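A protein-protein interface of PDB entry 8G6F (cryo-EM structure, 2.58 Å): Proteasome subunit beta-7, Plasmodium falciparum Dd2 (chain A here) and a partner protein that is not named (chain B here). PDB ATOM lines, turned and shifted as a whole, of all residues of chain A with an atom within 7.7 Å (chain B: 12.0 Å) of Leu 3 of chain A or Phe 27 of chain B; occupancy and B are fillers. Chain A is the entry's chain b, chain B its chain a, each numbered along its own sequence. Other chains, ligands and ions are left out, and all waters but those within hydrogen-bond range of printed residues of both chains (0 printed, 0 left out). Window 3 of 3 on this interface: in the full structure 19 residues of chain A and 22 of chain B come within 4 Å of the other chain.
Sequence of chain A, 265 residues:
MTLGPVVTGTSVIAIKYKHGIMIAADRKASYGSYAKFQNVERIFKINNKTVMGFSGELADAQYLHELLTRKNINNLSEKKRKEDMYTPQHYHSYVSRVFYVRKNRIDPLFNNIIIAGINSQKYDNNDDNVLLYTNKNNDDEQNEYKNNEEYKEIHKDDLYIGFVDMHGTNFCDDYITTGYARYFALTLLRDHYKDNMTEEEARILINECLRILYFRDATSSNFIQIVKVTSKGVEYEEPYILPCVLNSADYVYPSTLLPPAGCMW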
ATOM      1  N   THR A   2     -20.538 -27.740 -15.253  1.00  0.00           N
ATOM      2  CA  THR A   2     -21.725 -27.649 -16.089  1.00  0.00           C
ATOM      3  C   THR A   2     -21.784 -28.821 -17.055  1.00  0.00           C
ATOM      4  O   THR A   2     -20.965 -28.930 -17.963  1.00  0.00           O
ATOM      5  CB  THR A   2     -21.755 -26.336 -16.885  1.00  0.00           C
ATOM      6  OG1 THR A   2     -21.622 -25.228 -15.989  1.00  0.00           O
ATOM      7  CG2 THR A   2     -23.050 -26.202 -17.657  1.00  0.00           C
ATOM      8  N   LEU A   3     -22.759 -29.703 -16.849  1.00  0.00           N
ATOM      9  CA  LEU A   3     -22.933 -30.844 -17.735  1.00  0.00           C
ATOM     10  C   LEU A   3     -23.721 -30.497 -18.988  1.00  0.00           C
ATOM     11  O   LEU A   3     -23.642 -31.234 -19.974  1.00  0.00           O
ATOM     12  CB  LEU A   3     -23.632 -31.980 -16.988  1.00  0.00           C
ATOM     13  CG  LEU A   3     -22.947 -32.432 -15.699  1.00  0.00           C
ATOM     14  CD1 LEU A   3     -23.786 -33.482 -15.002  1.00  0.00           C
ATOM     15  CD2 LEU A   3     -21.553 -32.957 -15.985  1.00  0.00           C
ATOM     16  N   GLY A   4     -24.469 -29.402 -18.978  1.00  0.00           N
ATOM     17  CA  GLY A   4     -25.246 -29.009 -20.124  1.00  0.00           C
ATOM     18  C   GLY A   4     -26.029 -27.743 -19.867  1.00  0.00           C
ATOM     19  O   GLY A   4     -26.059 -27.217 -18.752  1.00  0.00           O
ATOM     20  N   PRO A   5     -26.679 -27.225 -20.904  1.00  0.00           N
ATOM     21  CA  PRO A   5     -27.451 -25.989 -20.756  1.00  0.00           C
ATOM     22  C   PRO A   5     -28.801 -26.222 -20.096  1.00  0.00           C
ATOM     23  O   PRO A   5     -29.505 -27.188 -20.397  1.00  0.00           O
ATOM     24  CB  PRO A   5     -27.619 -25.513 -22.201  1.00  0.00           C
ATOM     25  CG  PRO A   5     -27.561 -26.752 -23.010  1.00  0.00           C
ATOM     26  CD  PRO A   5     -26.659 -27.706 -22.295  1.00  0.00           C
ATOM     27  N   VAL A   6     -29.168 -25.310 -19.198  1.00  0.00           N
ATOM     28  CA  VAL A   6     -30.459 -25.373 -18.521  1.00  0.00           C
ATOM     29  C   VAL A   6     -31.228 -24.095 -18.820  1.00  0.00           C
ATOM     30  O   VAL A   6     -32.307 -24.134 -19.422  1.00  0.00           O
ATOM     31  CB  VAL A   6     -30.285 -25.577 -17.004  1.00  0.00           C
ATOM     32  CG1 VAL A   6     -31.616 -25.464 -16.299  1.00  0.00           C
ATOM     33  CG2 VAL A   6     -29.655 -26.922 -16.720  1.00  0.00           C
ATOM     34  N   GLU A  57     -25.605 -21.008 -22.009  1.00  0.00           N
ATOM     35  CA  GLU A  57     -25.941 -21.076 -20.593  1.00  0.00           C
ATOM     36  C   GLU A  57     -25.667 -19.746 -19.899  1.00  0.00           C
ATOM     37  O   GLU A  57     -24.556 -19.202 -19.960  1.00  0.00           O
ATOM     38  CB  GLU A  57     -25.163 -22.205 -19.920  1.00  0.00           C
ATOM     39  CG  GLU A  57     -25.298 -22.261 -18.402  1.00  0.00           C
ATOM     40  CD  GLU A  57     -26.731 -22.435 -17.929  1.00  0.00           C
ATOM     41  OE1 GLU A  57     -27.360 -23.453 -18.279  1.00  0.00           O
ATOM     42  OE2 GLU A  57     -27.229 -21.555 -17.199  1.00  0.00           O
ATOM     43  N   ASP A  60     -22.756 -19.866 -17.167  1.00  0.00           N
ATOM     44  CA  ASP A  60     -21.408 -19.781 -17.714  1.00  0.00           C
ATOM     45  C   ASP A  60     -21.132 -18.395 -18.274  1.00  0.00           C
ATOM     46  O   ASP A  60     -20.013 -17.879 -18.150  1.00  0.00           O
ATOM     47  CB  ASP A  60     -21.220 -20.849 -18.787  1.00  0.00           C
ATOM     48  CG  ASP A  60     -21.322 -22.253 -18.236  1.00  0.00           C
ATOM     49  OD1 ASP A  60     -21.044 -22.450 -17.039  1.00  0.00           O
ATOM     50  OD2 ASP A  60     -21.675 -23.165 -19.002  1.00  0.00           O
ATOM     51  N   ILE A 106     -12.081 -30.907 -20.842  1.00  0.00           N
ATOM     52  CA  ILE A 106     -13.415 -31.449 -21.080  1.00  0.00           C
ATOM     53  C   ILE A 106     -14.349 -30.940 -19.992  1.00  0.00           C
ATOM     54  O   ILE A 106     -15.172 -31.688 -19.455  1.00  0.00           O
ATOM     55  CB  ILE A 106     -13.398 -32.985 -21.147  1.00  0.00           C
ATOM     56  CG1 ILE A 106     -12.209 -33.455 -21.984  1.00  0.00           C
ATOM     57  CG2 ILE A 106     -14.687 -33.509 -21.759  1.00  0.00           C
ATOM     58  CD1 ILE A 106     -12.225 -34.926 -22.298  1.00  0.00           C
ATOM     59  N   ASP A 107     -14.216 -29.658 -19.662  1.00  0.00           N
ATOM     60  CA  ASP A 107     -15.104 -28.968 -18.728  1.00  0.00           C
ATOM     61  C   ASP A 107     -15.529 -27.646 -19.355  1.00  0.00           C
ATOM     62  O   ASP A 107     -15.235 -26.567 -18.834  1.00  0.00           O
ATOM     63  CB  ASP A 107     -14.405 -28.744 -17.388  1.00  0.00           C
ATOM     64  CG  ASP A 107     -15.375 -28.427 -16.264  1.00  0.00           C
ATOM     65  OD1 ASP A 107     -16.422 -29.100 -16.163  1.00  0.00           O
ATOM     66  OD2 ASP A 107     -15.091 -27.498 -15.481  1.00  0.00           O
ATOM     67  N   PRO A 108     -16.233 -27.696 -20.479  1.00  0.00           N
ATOM     68  CA  PRO A 108     -16.456 -26.489 -21.274  1.00  0.00           C
ATOM     69  C   PRO A 108     -17.512 -25.568 -20.684  1.00  0.00           C
ATOM     70  O   PRO A 108     -18.339 -25.956 -19.860  1.00  0.00           O
ATOM     71  CB  PRO A 108     -16.924 -27.049 -22.619  1.00  0.00           C
ATOM     72  CG  PRO A 108     -17.621 -28.294 -22.257  1.00  0.00           C
ATOM     73  CD  PRO A 108     -16.897 -28.868 -21.074  1.00  0.00           C
ATOM     74  N   PHE A 110     -20.784 -23.764 -21.803  1.00  0.00           N
ATOM     75  CA  PHE A 110     -21.783 -24.012 -22.840  1.00  0.00           C
ATOM     76  C   PHE A 110     -22.258 -22.673 -23.404  1.00  0.00           C
ATOM     77  O   PHE A 110     -23.360 -22.193 -23.137  1.00  0.00           O
ATOM     78  CB  PHE A 110     -22.929 -24.840 -22.281  1.00  0.00           C
ATOM     79  CG  PHE A 110     -22.617 -26.301 -22.188  1.00  0.00           C
ATOM     80  CD1 PHE A 110     -21.844 -26.792 -21.156  1.00  0.00           C
ATOM     81  CD2 PHE A 110     -23.081 -27.182 -23.143  1.00  0.00           C
ATOM     82  CE1 PHE A 110     -21.546 -28.130 -21.076  1.00  0.00           C
ATOM     83  CE2 PHE A 110     -22.785 -28.523 -23.067  1.00  0.00           C
ATOM     84  CZ  PHE A 110     -22.016 -28.996 -22.031  1.00  0.00           C
ATOM     85  N   MET A 166     -17.623 -23.230 -28.410  1.00  0.00           N
ATOM     86  CA  MET A 166     -17.412 -24.141 -27.288  1.00  0.00           C
ATOM     87  C   MET A 166     -16.090 -24.887 -27.395  1.00  0.00           C
ATOM     88  O   MET A 166     -15.460 -25.177 -26.373  1.00  0.00           O
ATOM     89  CB  MET A 166     -18.562 -25.141 -27.207  1.00  0.00           C
ATOM     90  CG  MET A 166     -19.835 -24.577 -26.603  1.00  0.00           C
ATOM     91  SD  MET A 166     -20.979 -25.828 -25.997  1.00  0.00           S
ATOM     92  CE  MET A 166     -19.950 -26.731 -24.852  1.00  0.00           C
ATOM     93  N   GLY B  26     -29.068 -37.075 -16.726  1.00  0.00           N
ATOM     94  CA  GLY B  26     -29.805 -37.146 -17.975  1.00  0.00           C
ATOM     95  C   GLY B  26     -29.289 -36.169 -19.013  1.00  0.00           C
ATOM     96  O   GLY B  26     -30.069 -35.533 -19.722  1.00  0.00           O
ATOM     97  N   PHE B  27     -27.967 -36.052 -19.098  1.00  0.00           N
ATOM     98  CA  PHE B  27     -27.307 -35.151 -20.030  1.00  0.00           C
ATOM     99  C   PHE B  27     -26.429 -35.952 -20.981  1.00  0.00           C
ATOM    100  O   PHE B  27     -25.954 -37.041 -20.650  1.00  0.00           O
ATOM    101  CB  PHE B  27     -26.449 -34.111 -19.291  1.00  0.00           C
ATOM    102  CG  PHE B  27     -27.126 -32.781 -19.093  1.00  0.00           C
ATOM    103  CD1 PHE B  27     -27.702 -32.109 -20.158  1.00  0.00           C
ATOM    104  CD2 PHE B  27     -27.171 -32.197 -17.840  1.00  0.00           C
ATOM    105  CE1 PHE B  27     -28.318 -30.887 -19.973  1.00  0.00           C
ATOM    106  CE2 PHE B  27     -27.784 -30.976 -17.652  1.00  0.00           C
ATOM    107  CZ  PHE B  27     -28.357 -30.321 -18.720  1.00  0.00           C
ATOM    108  N   LYS B  28     -26.219 -35.399 -22.169  1.00  0.00           N
ATOM    109  CA  LYS B  28     -25.368 -36.023 -23.169  1.00  0.00           C
ATOM    110  C   LYS B  28     -23.922 -35.595 -22.964  1.00  0.00           C
ATOM    111  O   LYS B  28     -23.646 -34.451 -22.598  1.00  0.00           O
ATOM    112  CB  LYS B  28     -25.824 -35.658 -24.583  1.00  0.00           C
ATOM    113  CG  LYS B  28     -26.095 -34.179 -24.806  1.00  0.00           C
ATOM    114  CD  LYS B  28     -26.625 -33.919 -26.205  1.00  0.00           C
ATOM    115  CE  LYS B  28     -28.145 -33.916 -26.227  1.00  0.00           C
ATOM    116  NZ  LYS B  28     -28.716 -32.689 -25.609  1.00  0.00           N
ATOM    117  N   ARG B  29     -23.002 -36.525 -23.196  1.00  0.00           N
ATOM    118  CA  ARG B  29     -21.587 -36.221 -23.070  1.00  0.00           C
ATOM    119  C   ARG B  29     -21.129 -35.310 -24.202  1.00  0.00           C
ATOM    120  O   ARG B  29     -21.648 -35.357 -25.318  1.00  0.00           O
ATOM    121  CB  ARG B  29     -20.764 -37.506 -23.072  1.00  0.00           C
ATOM    122  CG  ARG B  29     -19.527 -37.438 -22.202  1.00  0.00           C
ATOM    123  CD  ARG B  29     -18.597 -38.606 -22.469  1.00  0.00           C
ATOM    124  NE  ARG B  29     -18.227 -38.703 -23.876  1.00  0.00           N
ATOM    125  CZ  ARG B  29     -17.432 -37.851 -24.509  1.00  0.00           C
ATOM    126  NH1 ARG B  29     -16.882 -36.820 -23.885  1.00  0.00           N
ATOM    127  NH2 ARG B  29     -17.179 -38.037 -25.798  1.00  0.00           N
ATOM    128  N   TRP B  30     -20.139 -34.476 -23.901  1.00  0.00           N
ATOM    129  CA  TRP B  30     -19.618 -33.497 -24.844  1.00  0.00           C
ATOM    130  C   TRP B  30     -18.348 -34.036 -25.483  1.00  0.00           C
ATOM    131  O   TRP B  30     -17.431 -34.472 -24.780  1.00  0.00           O
ATOM    132  CB  TRP B  30     -19.340 -32.170 -24.139  1.00  0.00           C
ATOM    133  CG  TRP B  30     -18.806 -31.103 -25.033  1.00  0.00           C
ATOM    134  CD1 TRP B  30     -19.497 -30.400 -25.969  1.00  0.00           C
ATOM    135  CD2 TRP B  30     -17.460 -30.618 -25.077  1.00  0.00           C
ATOM    136  NE1 TRP B  30     -18.669 -29.504 -26.593  1.00  0.00           N
ATOM    137  CE2 TRP B  30     -17.412 -29.617 -26.061  1.00  0.00           C
ATOM    138  CE3 TRP B  30     -16.293 -30.929 -24.375  1.00  0.00           C
ATOM    139  CZ2 TRP B  30     -16.246 -28.926 -26.365  1.00  0.00           C
ATOM    140  CZ3 TRP B  30     -15.139 -30.243 -24.677  1.00  0.00           C
ATOM    141  CH2 TRP B  30     -15.122 -29.253 -25.664  1.00  0.00           C
ATOM    142  N   TYR B  31     -18.303 -34.012 -26.813  1.00  0.00           N
ATOM    143  CA  TYR B  31     -17.149 -34.502 -27.551  1.00  0.00           C
ATOM    144  C   TYR B  31     -16.172 -33.357 -27.782  1.00  0.00           C
ATOM    145  O   TYR B  31     -16.562 -32.341 -28.370  1.00  0.00           O
ATOM    146  CB  TYR B  31     -17.583 -35.096 -28.879  1.00  0.00           C
ATOM    147  CG  TYR B  31     -16.562 -35.999 -29.531  1.00  0.00           C
ATOM    148  CD1 TYR B  31     -16.010 -37.068 -28.842  1.00  0.00           C
ATOM    149  CD2 TYR B  31     -16.154 -35.786 -30.840  1.00  0.00           C
ATOM    150  CE1 TYR B  31     -15.079 -37.896 -29.436  1.00  0.00           C
ATOM    151  CE2 TYR B  31     -15.226 -36.609 -31.442  1.00  0.00           C
ATOM    152  CZ  TYR B  31     -14.691 -37.661 -30.736  1.00  0.00           C
ATOM    153  OH  TYR B  31     -13.764 -38.482 -31.332  1.00  0.00           O
ATOM    154  N   PRO B  32     -14.916 -33.466 -27.349  1.00  0.00           N
ATOM    155  CA  PRO B  32     -13.987 -32.337 -27.448  1.00  0.00           C
ATOM    156  C   PRO B  32     -13.318 -32.164 -28.802  1.00  0.00           C
ATOM    157  O   PRO B  32     -12.354 -31.402 -28.891  1.00  0.00           O
ATOM    158  CB  PRO B  32     -12.947 -32.685 -26.376  1.00  0.00           C
ATOM    159  CG  PRO B  32     -12.890 -34.148 -26.418  1.00  0.00           C
ATOM    160  CD  PRO B  32     -14.303 -34.598 -26.633  1.00  0.00           C
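CB of Leu 3 of chain A touches CD2 of Phe 27 of chain B, 3.6 Å away. Gly 4 of chain A touches Phe 27 of chain B. Pro 5 of chain A touches Phe 27 of chain B. CG of Pro 108 of chain A touches CE3 of Trp 30 of chain B, at 3.6 Å. Trp 30 of chain B touches Met 166 of chain A (NE1 to CE, 3.5 Å).
No residue of chain B comes within 4 Å of Thr 2 of chain A. Of chain B, only Phe 27 comes within 4 Å of Leu 3 of chain A. Pro 5 of chain A touches just one residue of chain B: Phe 27 (3.7 Å). Of the printed residues of chain B, Pro 108 of chain A touches Trp 30. Printed residues of chain B within 4 Å of Met 166 of chain A: Trp 30 (3.5 Å). No residue of chain A comes within 4 Å of Gly 26 of chain B. Of chain A, only Leu 3, Gly 4 and Pro 5 come within 4 Å of Phe 27 of chain B. The nearest printed residue of chain A that does not touch Trp 30 of chain B is Ile 106 of chain A (4.01 Å).
Printed residues of chain B that touch a printed residue of chain A: Phe 27 and Trp 30. Among the printed residues, 5 pairs touch across the chains.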
